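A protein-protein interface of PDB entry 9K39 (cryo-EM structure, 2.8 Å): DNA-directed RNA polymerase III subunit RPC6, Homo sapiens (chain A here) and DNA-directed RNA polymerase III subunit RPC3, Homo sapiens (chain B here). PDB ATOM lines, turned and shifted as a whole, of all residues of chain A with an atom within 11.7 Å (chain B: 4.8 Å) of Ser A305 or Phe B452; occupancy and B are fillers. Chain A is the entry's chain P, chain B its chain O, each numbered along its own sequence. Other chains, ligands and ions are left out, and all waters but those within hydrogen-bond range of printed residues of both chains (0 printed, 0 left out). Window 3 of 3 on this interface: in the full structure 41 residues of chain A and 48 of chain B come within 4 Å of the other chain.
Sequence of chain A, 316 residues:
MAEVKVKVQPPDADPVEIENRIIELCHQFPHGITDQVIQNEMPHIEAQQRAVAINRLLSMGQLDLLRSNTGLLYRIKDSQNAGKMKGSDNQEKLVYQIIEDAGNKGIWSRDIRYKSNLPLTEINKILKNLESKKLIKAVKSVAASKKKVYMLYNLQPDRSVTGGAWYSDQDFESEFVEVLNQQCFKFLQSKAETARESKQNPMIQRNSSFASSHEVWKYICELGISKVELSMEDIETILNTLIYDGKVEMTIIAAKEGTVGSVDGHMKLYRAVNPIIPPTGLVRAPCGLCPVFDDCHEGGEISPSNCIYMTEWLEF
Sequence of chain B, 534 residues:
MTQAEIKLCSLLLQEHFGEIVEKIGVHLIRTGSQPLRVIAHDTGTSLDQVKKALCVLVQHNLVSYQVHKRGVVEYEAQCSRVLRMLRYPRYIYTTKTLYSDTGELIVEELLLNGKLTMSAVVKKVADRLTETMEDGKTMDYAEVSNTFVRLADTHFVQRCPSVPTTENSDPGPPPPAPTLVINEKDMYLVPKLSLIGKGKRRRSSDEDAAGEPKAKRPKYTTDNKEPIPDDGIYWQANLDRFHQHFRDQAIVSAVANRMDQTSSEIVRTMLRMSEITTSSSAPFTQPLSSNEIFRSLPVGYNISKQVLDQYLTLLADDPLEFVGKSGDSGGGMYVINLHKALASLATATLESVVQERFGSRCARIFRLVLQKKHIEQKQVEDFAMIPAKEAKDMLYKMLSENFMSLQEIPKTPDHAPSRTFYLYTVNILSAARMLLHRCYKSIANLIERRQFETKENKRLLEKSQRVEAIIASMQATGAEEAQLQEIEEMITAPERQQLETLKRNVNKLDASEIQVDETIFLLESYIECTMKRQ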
ATOM      1  N   PRO A 286     -10.825  -5.857  -8.609  1.00  0.00           N
ATOM      2  CA  PRO A 286      -9.394  -6.060  -8.320  1.00  0.00           C
ATOM      3  C   PRO A 286      -8.666  -4.784  -7.941  1.00  0.00           C
ATOM      4  O   PRO A 286      -7.638  -4.849  -7.255  1.00  0.00           O
ATOM      5  CB  PRO A 286      -8.855  -6.652  -9.630  1.00  0.00           C
ATOM      6  CG  PRO A 286     -10.052  -7.234 -10.311  1.00  0.00           C
ATOM      7  CD  PRO A 286     -11.191  -6.328  -9.954  1.00  0.00           C
ATOM      8  N   CYS A 287      -9.164  -3.622  -8.371  1.00  0.00           N
ATOM      9  CA  CYS A 287      -8.490  -2.365  -8.064  1.00  0.00           C
ATOM     10  C   CYS A 287      -8.552  -2.039  -6.577  1.00  0.00           C
ATOM     11  O   CYS A 287      -7.630  -1.415  -6.040  1.00  0.00           O
ATOM     12  CB  CYS A 287      -9.107  -1.227  -8.877  1.00  0.00           C
ATOM     13  SG  CYS A 287      -9.498  -1.654 -10.591  1.00  0.00           S
ATOM     14  N   ASP A 295       1.079   2.709  -7.579  1.00  0.00           N
ATOM     15  CA  ASP A 295       1.869   2.804  -8.802  1.00  0.00           C
ATOM     16  C   ASP A 295       1.036   2.672 -10.070  1.00  0.00           C
ATOM     17  O   ASP A 295       1.611   2.537 -11.157  1.00  0.00           O
ATOM     18  CB  ASP A 295       2.969   1.739  -8.797  1.00  0.00           C
ATOM     19  CG  ASP A 295       3.913   1.885  -7.620  1.00  0.00           C
ATOM     20  OD1 ASP A 295       4.002   2.999  -7.061  1.00  0.00           O
ATOM     21  OD2 ASP A 295       4.576   0.889  -7.258  1.00  0.00           O
ATOM     22  N   CYS A 296      -0.292   2.699  -9.969  1.00  0.00           N
ATOM     23  CA  CYS A 296      -1.138   2.590 -11.149  1.00  0.00           C
ATOM     24  C   CYS A 296      -1.041   3.853 -11.996  1.00  0.00           C
ATOM     25  O   CYS A 296      -1.044   4.969 -11.470  1.00  0.00           O
ATOM     26  CB  CYS A 296      -2.589   2.344 -10.741  1.00  0.00           C
ATOM     27  SG  CYS A 296      -3.767   2.479 -12.108  1.00  0.00           S
ATOM     28  N   HIS A 297      -0.963   3.672 -13.314  1.00  0.00           N
ATOM     29  CA  HIS A 297      -0.912   4.793 -14.242  1.00  0.00           C
ATOM     30  C   HIS A 297      -1.446   4.345 -15.593  1.00  0.00           C
ATOM     31  O   HIS A 297      -1.463   3.152 -15.912  1.00  0.00           O
ATOM     32  CB  HIS A 297       0.511   5.347 -14.378  1.00  0.00           C
ATOM     33  CG  HIS A 297       0.593   6.622 -15.161  1.00  0.00           C
ATOM     34  ND1 HIS A 297      -0.186   7.722 -14.872  1.00  0.00           N
ATOM     35  CD2 HIS A 297       1.356   6.969 -16.224  1.00  0.00           C
ATOM     36  CE1 HIS A 297       0.096   8.693 -15.721  1.00  0.00           C
ATOM     37  NE2 HIS A 297       1.030   8.263 -16.553  1.00  0.00           N
ATOM     38  N   GLU A 298      -1.890   5.323 -16.385  1.00  0.00           N
ATOM     39  CA  GLU A 298      -2.415   5.034 -17.716  1.00  0.00           C
ATOM     40  C   GLU A 298      -1.332   4.453 -18.619  1.00  0.00           C
ATOM     41  O   GLU A 298      -1.437   3.314 -19.089  1.00  0.00           O
ATOM     42  CB  GLU A 298      -3.008   6.306 -18.330  1.00  0.00           C
ATOM     43  CG  GLU A 298      -3.566   6.122 -19.729  1.00  0.00           C
ATOM     44  CD  GLU A 298      -4.102   7.411 -20.318  1.00  0.00           C
ATOM     45  OE1 GLU A 298      -4.004   8.459 -19.647  1.00  0.00           O
ATOM     46  OE2 GLU A 298      -4.622   7.376 -21.452  1.00  0.00           O
ATOM     47  N   GLY A 299      -0.281   5.226 -18.875  1.00  0.00           N
ATOM     48  CA  GLY A 299       0.811   4.767 -19.713  1.00  0.00           C
ATOM     49  C   GLY A 299       2.057   4.416 -18.928  1.00  0.00           C
ATOM     50  O   GLY A 299       2.765   5.305 -18.447  1.00  0.00           O
ATOM     51  N   GLY A 300       2.335   3.125 -18.794  1.00  0.00           N
ATOM     52  CA  GLY A 300       3.503   2.697 -18.053  1.00  0.00           C
ATOM     53  C   GLY A 300       3.558   1.189 -17.957  1.00  0.00           C
ATOM     54  O   GLY A 300       2.839   0.476 -18.661  1.00  0.00           O
ATOM     55  N   GLU A 301       4.437   0.713 -17.072  1.00  0.00           N
ATOM     56  CA  GLU A 301       4.569  -0.726 -16.869  1.00  0.00           C
ATOM     57  C   GLU A 301       3.328  -1.307 -16.200  1.00  0.00           C
ATOM     58  O   GLU A 301       2.872  -2.395 -16.565  1.00  0.00           O
ATOM     59  CB  GLU A 301       5.817  -1.022 -16.038  1.00  0.00           C
ATOM     60  CG  GLU A 301       7.104  -0.470 -16.628  1.00  0.00           C
ATOM     61  CD  GLU A 301       8.311  -0.764 -15.763  1.00  0.00           C
ATOM     62  OE1 GLU A 301       8.182  -1.560 -14.810  1.00  0.00           O
ATOM     63  OE2 GLU A 301       9.391  -0.194 -16.034  1.00  0.00           O
ATOM     64  N   ILE A 302       2.769  -0.593 -15.229  1.00  0.00           N
ATOM     65  CA  ILE A 302       1.578  -1.027 -14.510  1.00  0.00           C
ATOM     66  C   ILE A 302       0.410  -0.220 -15.061  1.00  0.00           C
ATOM     67  O   ILE A 302       0.191   0.932 -14.669  1.00  0.00           O
ATOM     68  CB  ILE A 302       1.723  -0.849 -12.993  1.00  0.00           C
ATOM     69  CG1 ILE A 302       2.939  -1.621 -12.483  1.00  0.00           C
ATOM     70  CG2 ILE A 302       0.461  -1.313 -12.280  1.00  0.00           C
ATOM     71  CD1 ILE A 302       3.175  -1.478 -10.996  1.00  0.00           C
ATOM     72  N   SER A 303      -0.344  -0.823 -15.973  1.00  0.00           N
ATOM     73  CA  SER A 303      -1.471  -0.175 -16.618  1.00  0.00           C
ATOM     74  C   SER A 303      -2.704  -1.059 -16.507  1.00  0.00           C
ATOM     75  O   SER A 303      -2.595  -2.288 -16.496  1.00  0.00           O
ATOM     76  CB  SER A 303      -1.172   0.109 -18.099  1.00  0.00           C
ATOM     77  OG  SER A 303      -2.277   0.717 -18.744  1.00  0.00           O
ATOM     78  N   PRO A 304      -3.893  -0.457 -16.408  1.00  0.00           N
ATOM     79  CA  PRO A 304      -5.117  -1.272 -16.379  1.00  0.00           C
ATOM     80  C   PRO A 304      -5.331  -2.084 -17.644  1.00  0.00           C
ATOM     81  O   PRO A 304      -6.004  -3.120 -17.599  1.00  0.00           O
ATOM     82  CB  PRO A 304      -6.230  -0.232 -16.175  1.00  0.00           C
ATOM     83  CG  PRO A 304      -5.627   1.068 -16.608  1.00  0.00           C
ATOM     84  CD  PRO A 304      -4.182   0.976 -16.238  1.00  0.00           C
ATOM     85  N   SER A 305      -4.782  -1.645 -18.779  1.00  0.00           N
ATOM     86  CA  SER A 305      -4.957  -2.390 -20.019  1.00  0.00           C
ATOM     87  C   SER A 305      -4.250  -3.739 -19.962  1.00  0.00           C
ATOM     88  O   SER A 305      -4.801  -4.756 -20.397  1.00  0.00           O
ATOM     89  CB  SER A 305      -4.444  -1.568 -21.200  1.00  0.00           C
ATOM     90  OG  SER A 305      -3.078  -1.225 -21.028  1.00  0.00           O
ATOM     91  N   ASN A 306      -3.031  -3.770 -19.421  1.00  0.00           N
ATOM     92  CA  ASN A 306      -2.250  -4.997 -19.321  1.00  0.00           C
ATOM     93  C   ASN A 306      -2.165  -5.519 -17.889  1.00  0.00           C
ATOM     94  O   ASN A 306      -1.152  -6.117 -17.509  1.00  0.00           O
ATOM     95  CB  ASN A 306      -0.849  -4.787 -19.900  1.00  0.00           C
ATOM     96  CG  ASN A 306      -0.155  -3.562 -19.329  1.00  0.00           C
ATOM     97  OD1 ASN A 306      -0.478  -3.098 -18.239  1.00  0.00           O
ATOM     98  ND2 ASN A 306       0.812  -3.033 -20.073  1.00  0.00           N
ATOM     99  N   CYS A 307      -3.203  -5.298 -17.088  1.00  0.00           N
ATOM    100  CA  CYS A 307      -3.197  -5.752 -15.704  1.00  0.00           C
ATOM    101  C   CYS A 307      -3.349  -7.266 -15.633  1.00  0.00           C
ATOM    102  O   CYS A 307      -4.112  -7.863 -16.397  1.00  0.00           O
ATOM    103  CB  CYS A 307      -4.318  -5.075 -14.919  1.00  0.00           C
ATOM    104  SG  CYS A 307      -4.527  -5.696 -13.237  1.00  0.00           S
ATOM    105  N   ILE A 308      -2.608  -7.889 -14.711  1.00  0.00           N
ATOM    106  CA  ILE A 308      -2.722  -9.331 -14.517  1.00  0.00           C
ATOM    107  C   ILE A 308      -3.866  -9.652 -13.561  1.00  0.00           C
ATOM    108  O   ILE A 308      -4.549 -10.675 -13.710  1.00  0.00           O
ATOM    109  CB  ILE A 308      -1.382  -9.908 -14.022  1.00  0.00           C
ATOM    110  CG1 ILE A 308      -0.255  -9.539 -14.989  1.00  0.00           C
ATOM    111  CG2 ILE A 308      -1.471 -11.418 -13.863  1.00  0.00           C
ATOM    112  CD1 ILE A 308      -0.456 -10.065 -16.394  1.00  0.00           C
ATOM    113  N   TYR A 309      -4.094  -8.787 -12.568  1.00  0.00           N
ATOM    114  CA  TYR A 309      -5.168  -9.022 -11.605  1.00  0.00           C
ATOM    115  C   TYR A 309      -6.525  -9.065 -12.295  1.00  0.00           C
ATOM    116  O   TYR A 309      -7.290 -10.021 -12.128  1.00  0.00           O
ATOM    117  CB  TYR A 309      -5.157  -7.941 -10.525  1.00  0.00           C
ATOM    118  CG  TYR A 309      -3.867  -7.847  -9.747  1.00  0.00           C
ATOM    119  CD1 TYR A 309      -3.633  -8.668  -8.652  1.00  0.00           C
ATOM    120  CD2 TYR A 309      -2.887  -6.927 -10.098  1.00  0.00           C
ATOM    121  CE1 TYR A 309      -2.458  -8.582  -7.935  1.00  0.00           C
ATOM    122  CE2 TYR A 309      -1.706  -6.836  -9.386  1.00  0.00           C
ATOM    123  CZ  TYR A 309      -1.498  -7.666  -8.306  1.00  0.00           C
ATOM    124  OH  TYR A 309      -0.327  -7.579  -7.593  1.00  0.00           O
ATOM    125  N   MET A 310      -6.839  -8.029 -13.078  1.00  0.00           N
ATOM    126  CA  MET A 310      -8.113  -8.006 -13.786  1.00  0.00           C
ATOM    127  C   MET A 310      -8.188  -9.101 -14.844  1.00  0.00           C
ATOM    128  O   MET A 310      -9.275  -9.621 -15.111  1.00  0.00           O
ATOM    129  CB  MET A 310      -8.344  -6.632 -14.411  1.00  0.00           C
ATOM    130  CG  MET A 310      -8.646  -5.549 -13.387  1.00  0.00           C
ATOM    131  SD  MET A 310      -9.124  -3.980 -14.126  1.00  0.00           S
ATOM    132  CE  MET A 310      -7.598  -3.508 -14.918  1.00  0.00           C
ATOM    133  N   THR A 311      -7.054  -9.474 -15.435  1.00  0.00           N
ATOM    134  CA  THR A 311      -7.049 -10.571 -16.399  1.00  0.00           C
ATOM    135  C   THR A 311      -7.474 -11.878 -15.740  1.00  0.00           C
ATOM    136  O   THR A 311      -8.362 -12.582 -16.240  1.00  0.00           O
ATOM    137  CB  THR A 311      -5.661 -10.714 -17.027  1.00  0.00           C
ATOM    138  OG1 THR A 311      -5.311  -9.492 -17.691  1.00  0.00           O
ATOM    139  CG2 THR A 311      -5.646 -11.854 -18.034  1.00  0.00           C
ATOM    140  N   GLU A 312      -6.848 -12.222 -14.610  1.00  0.00           N
ATOM    141  CA  GLU A 312      -7.218 -13.441 -13.900  1.00  0.00           C
ATOM    142  C   GLU A 312      -8.639 -13.355 -13.355  1.00  0.00           C
ATOM    143  O   GLU A 312      -9.345 -14.366 -13.279  1.00  0.00           O
ATOM    144  CB  GLU A 312      -6.223 -13.715 -12.770  1.00  0.00           C
ATOM    145  CG  GLU A 312      -4.794 -13.924 -13.240  1.00  0.00           C
ATOM    146  CD  GLU A 312      -3.830 -14.131 -12.087  1.00  0.00           C
ATOM    147  OE1 GLU A 312      -4.283 -14.115 -10.922  1.00  0.00           O
ATOM    148  OE2 GLU A 312      -2.623 -14.311 -12.347  1.00  0.00           O
ATOM    149  N   TRP A 313      -9.070 -12.155 -12.957  1.00  0.00           N
ATOM    150  CA  TRP A 313     -10.414 -11.990 -12.414  1.00  0.00           C
ATOM    151  C   TRP A 313     -11.479 -12.190 -13.488  1.00  0.00           C
ATOM    152  O   TRP A 313     -12.515 -12.816 -13.230  1.00  0.00           O
ATOM    153  CB  TRP A 313     -10.533 -10.613 -11.766  1.00  0.00           C
ATOM    154  CG  TRP A 313     -11.918 -10.225 -11.365  1.00  0.00           C
ATOM    155  CD1 TRP A 313     -12.700 -10.824 -10.420  1.00  0.00           C
ATOM    156  CD2 TRP A 313     -12.682  -9.129 -11.878  1.00  0.00           C
ATOM    157  NE1 TRP A 313     -13.908 -10.176 -10.325  1.00  0.00           N
ATOM    158  CE2 TRP A 313     -13.920  -9.132 -11.210  1.00  0.00           C
ATOM    159  CE3 TRP A 313     -12.437  -8.149 -12.846  1.00  0.00           C
ATOM    160  CZ2 TRP A 313     -14.911  -8.191 -11.476  1.00  0.00           C
ATOM    161  CZ3 TRP A 313     -13.422  -7.218 -13.110  1.00  0.00           C
ATOM    162  CH2 TRP A 313     -14.644  -7.246 -12.428  1.00  0.00           C
ATOM    163  N   LEU A 314     -11.244 -11.673 -14.694  1.00  0.00           N
ATOM    164  CA  LEU A 314     -12.192 -11.873 -15.785  1.00  0.00           C
ATOM    165  C   LEU A 314     -12.135 -13.304 -16.314  1.00  0.00           C
ATOM    166  O   LEU A 314     -13.157 -13.856 -16.738  1.00  0.00           O
ATOM    167  CB  LEU A 314     -11.922 -10.873 -16.910  1.00  0.00           C
ATOM    168  CG  LEU A 314     -12.166  -9.397 -16.585  1.00  0.00           C
ATOM    169  CD1 LEU A 314     -11.808  -8.518 -17.774  1.00  0.00           C
ATOM    170  CD2 LEU A 314     -13.609  -9.171 -16.163  1.00  0.00           C
ATOM    171  N   GLU B 448     -11.217   2.152 -18.184  1.00  0.00           N
ATOM    172  CA  GLU B 448     -10.076   2.105 -19.093  1.00  0.00           C
ATOM    173  C   GLU B 448      -9.850   0.696 -19.624  1.00  0.00           C
ATOM    174  O   GLU B 448      -9.579   0.510 -20.815  1.00  0.00           O
ATOM    175  CB  GLU B 448      -8.824   2.624 -18.388  1.00  0.00           C
ATOM    176  CG  GLU B 448      -7.572   2.624 -19.256  1.00  0.00           C
ATOM    177  CD  GLU B 448      -7.652   3.614 -20.401  1.00  0.00           C
ATOM    178  OE1 GLU B 448      -8.425   4.591 -20.296  1.00  0.00           O
ATOM    179  OE2 GLU B 448      -6.941   3.417 -21.410  1.00  0.00           O
ATOM    180  N   ARG B 449      -9.965  -0.312 -18.755  1.00  0.00           N
ATOM    181  CA  ARG B 449      -9.788  -1.693 -19.191  1.00  0.00           C
ATOM    182  C   ARG B 449     -10.887  -2.110 -20.162  1.00  0.00           C
ATOM    183  O   ARG B 449     -10.623  -2.805 -21.150  1.00  0.00           O
ATOM    184  CB  ARG B 449      -9.753  -2.624 -17.981  1.00  0.00           C
ATOM    185  CG  ARG B 449      -9.617  -4.101 -18.331  1.00  0.00           C
ATOM    186  CD  ARG B 449      -8.384  -4.360 -19.182  1.00  0.00           C
ATOM    187  NE  ARG B 449      -8.181  -5.783 -19.436  1.00  0.00           N
ATOM    188  CZ  ARG B 449      -7.446  -6.581 -18.670  1.00  0.00           C
ATOM    189  NH1 ARG B 449      -6.837  -6.096 -17.595  1.00  0.00           N
ATOM    190  NH2 ARG B 449      -7.316  -7.865 -18.977  1.00  0.00           N
ATOM    191  N   ARG B 450     -12.130  -1.698 -19.894  1.00  0.00           N
ATOM    192  CA  ARG B 450     -13.219  -2.018 -20.810  1.00  0.00           C
ATOM    193  C   ARG B 450     -12.996  -1.377 -22.174  1.00  0.00           C
ATOM    194  O   ARG B 450     -13.179  -2.026 -23.212  1.00  0.00           O
ATOM    195  CB  ARG B 450     -14.561  -1.573 -20.227  1.00  0.00           C
ATOM    196  CG  ARG B 450     -15.760  -2.061 -21.025  1.00  0.00           C
ATOM    197  CD  ARG B 450     -17.024  -1.284 -20.694  1.00  0.00           C
ATOM    198  NE  ARG B 450     -17.000   0.069 -21.245  1.00  0.00           N
ATOM    199  CZ  ARG B 450     -16.695   1.157 -20.548  1.00  0.00           C
ATOM    200  NH1 ARG B 450     -16.389   1.061 -19.263  1.00  0.00           N
ATOM    201  NH2 ARG B 450     -16.701   2.346 -21.138  1.00  0.00           N
ATOM    202  N   GLN B 451     -12.597  -0.104 -22.193  1.00  0.00           N
ATOM    203  CA  GLN B 451     -12.340   0.569 -23.461  1.00  0.00           C
ATOM    204  C   GLN B 451     -11.162  -0.064 -24.193  1.00  0.00           C
ATOM    205  O   GLN B 451     -11.178  -0.176 -25.422  1.00  0.00           O
ATOM    206  CB  GLN B 451     -12.094   2.059 -23.225  1.00  0.00           C
ATOM    207  CG  GLN B 451     -13.318   2.813 -22.727  1.00  0.00           C
ATOM    208  CD  GLN B 451     -13.055   4.291 -22.524  1.00  0.00           C
ATOM    209  OE1 GLN B 451     -11.946   4.777 -22.758  1.00  0.00           O
ATOM    210  NE2 GLN B 451     -14.076   5.019 -22.084  1.00  0.00           N
ATOM    211  N   PHE B 452     -10.138  -0.498 -23.452  1.00  0.00           N
ATOM    212  CA  PHE B 452      -9.000  -1.165 -24.079  1.00  0.00           C
ATOM    213  C   PHE B 452      -9.415  -2.488 -24.708  1.00  0.00           C
ATOM    214  O   PHE B 452      -9.006  -2.802 -25.833  1.00  0.00           O
ATOM    215  CB  PHE B 452      -7.891  -1.385 -23.049  1.00  0.00           C
ATOM    216  CG  PHE B 452      -6.775  -2.261 -23.540  1.00  0.00           C
ATOM    217  CD1 PHE B 452      -5.816  -1.765 -24.407  1.00  0.00           C
ATOM    218  CD2 PHE B 452      -6.679  -3.580 -23.126  1.00  0.00           C
ATOM    219  CE1 PHE B 452      -4.787  -2.568 -24.859  1.00  0.00           C
ATOM    220  CE2 PHE B 452      -5.650  -4.389 -23.573  1.00  0.00           C
ATOM    221  CZ  PHE B 452      -4.703  -3.880 -24.441  1.00  0.00           C
ATOM    222  N   GLU B 453     -10.217  -3.283 -23.994  1.00  0.00           N
ATOM    223  CA  GLU B 453     -10.681  -4.550 -24.550  1.00  0.00           C
ATOM    224  C   GLU B 453     -11.584  -4.325 -25.757  1.00  0.00           C
ATOM    225  O   GLU B 453     -11.569  -5.114 -26.710  1.00  0.00           O
ATOM    226  CB  GLU B 453     -11.403  -5.368 -23.480  1.00  0.00           C
ATOM    227  CG  GLU B 453     -10.484  -5.952 -22.421  1.00  0.00           C
ATOM    228  CD  GLU B 453     -11.182  -6.973 -21.543  1.00  0.00           C
ATOM    229  OE1 GLU B 453     -12.405  -7.159 -21.703  1.00  0.00           O
ATOM    230  OE2 GLU B 453     -10.505  -7.593 -20.696  1.00  0.00           O
ATOM    231  N   THR B 454     -12.388  -3.258 -25.730  1.00  0.00           N
ATOM    232  CA  THR B 454     -13.231  -2.943 -26.878  1.00  0.00           C
ATOM    233  C   THR B 454     -12.393  -2.531 -28.082  1.00  0.00           C
ATOM    234  O   THR B 454     -12.668  -2.945 -29.215  1.00  0.00           O
ATOM    235  CB  THR B 454     -14.224  -1.839 -26.511  1.00  0.00           C
ATOM    236  OG1 THR B 454     -14.985  -2.241 -25.361  1.00  0.00           O
ATOM    237  CG2 THR B 454     -15.170  -1.562 -27.667  1.00  0.00           C
ATOM    238  N   LYS B 455     -11.358  -1.714 -27.858  1.00  0.00           N
ATOM    239  CA  LYS B 455     -10.553  -1.209 -28.964  1.00  0.00           C
ATOM    240  C   LYS B 455      -9.665  -2.298 -29.557  1.00  0.00           C
ATOM    241  O   LYS B 455      -9.496  -2.367 -30.780  1.00  0.00           O
ATOM    242  CB  LYS B 455      -9.708  -0.025 -28.494  1.00  0.00           C
ATOM    243  CG  LYS B 455      -8.816   0.578 -29.569  1.00  0.00           C
ATOM    244  CD  LYS B 455      -7.987   1.726 -29.016  1.00  0.00           C
ATOM    245  CE  LYS B 455      -7.095   1.263 -27.874  1.00  0.00           C
ATOM    246  NZ  LYS B 455      -6.296   2.384 -27.303  1.00  0.00           N
ATOM    247  N   GLU B 456      -9.094  -3.161 -28.711  1.00  0.00           N
ATOM    248  CA  GLU B 456      -8.188  -4.188 -29.216  1.00  0.00           C
ATOM    249  C   GLU B 456      -8.926  -5.247 -30.020  1.00  0.00           C
ATOM    250  O   GLU B 456      -8.321  -5.916 -30.866  1.00  0.00           O
ATOM    251  CB  GLU B 456      -7.424  -4.837 -28.059  1.00  0.00           C
ATOM    252  CG  GLU B 456      -8.289  -5.675 -27.131  1.00  0.00           C
ATOM    253  CD  GLU B 456      -7.485  -6.370 -26.053  1.00  0.00           C
ATOM    254  OE1 GLU B 456      -6.240  -6.263 -26.074  1.00  0.00           O
ATOM    255  OE2 GLU B 456      -8.096  -7.023 -25.181  1.00  0.00           O
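The backbone NH (N) of Met A310 sits close to the side-chain sulfur (SG) of Cys A307, 3.3 Å away.
The side-chain sulfur of Cys A307 sits close to the backbone NH of Tyr A309 (3.2 Å).
NE of Arg B449 is in salt-bridge range of OE2 of Glu B453 (3.2 Å).
The side-chain hydroxyl of Ser A303 sits at hydrogen-bond distance from the side-chain hydroxyl of Ser A305 (3.1 Å).
O of Cys A307 lies within hydrogen-bond range of OG1 of Thr A311, 2.4 Å away.
Of the 9 printed residues of chain B, 4 touch a printed residue of chain A.
Printed residues of chain B that touch a printed residue of chain A: Glu B448, Arg B449, Phe B452 and Glu B453.
Hydrophobic or aromatic side chains of chain B within 4 Å of the printed part of chain A: Phe B452.
Hydrophobic or aromatic side chains of chain A that line the printed part of chain B: Pro A304, Met A310 and Leu A314.
Among the printed residues, no Asp or Glu carboxylate lies within 4 Å of a Lys or Arg side-chain nitrogen of the other chain.
Of the printed residues of chain B, Pro A304 touches Glu B448 (3.6 Å) and Arg B449 (3.1 Å).
Ser A305 touches just these residues of chain B: Arg B449 and Phe B452.
Printed residues of chain B within 4 Å of Cys A307: Arg B449 (3.5 Å).
Of the printed residues of chain B, Met A310 touches Arg B449.
Of the printed residues of chain B, Thr A311 touches Arg B449.
Trp A313 touches none of the printed residues of chain B.
Printed residues of chain B within 4 Å of Leu A314: Glu B453.
Glu B448 touches one residue of chain A.
Of chain A, only Pro A304 (3.1 Å), Ser A305 (3.6 Å), Cys A307 (3.5 Å), Met A310 (3.6 Å) and Thr A311 (2.9 Å) come within 4 Å of Arg B449.
No residue of chain A comes within 4 Å of Gln B451.
Phe B452 touches one residue of chain A.
No residue of chain A comes within 4 Å of Thr B454.
No residue of chain A comes within 4 Å of Lys B455.
The nearest residue of chain A that does not touch Phe B452 is Asn A306 (4.9 Å).
The nearest printed residue of chain B that does not touch Met A310 is Glu B453 (6.1 Å).
The guanidinium group (NH2) of Arg B449 sits at hydrogen-bond distance from the side-chain hydroxyl (OG1) of Thr A311 (2.9 Å).
NH1 of Arg B449 is in hydrogen-bond range of O of Cys A307 (3.5 Å).
NH1 of Arg B449 lies within hydrogen-bond range of O of Pro A304 (3.1 Å).
Pro A304 touches Glu B448 (CG to CG, 3.6 Å).
Arg B449 touches Ser A305 (CZ to O, 3.6 Å).
Phe B452 touches Ser A305 (CE2 to O, 3.3 Å).
Met A310 touches Arg B449 (CB to NH1, 3.6 Å).
Leu A314 touches Glu B453.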
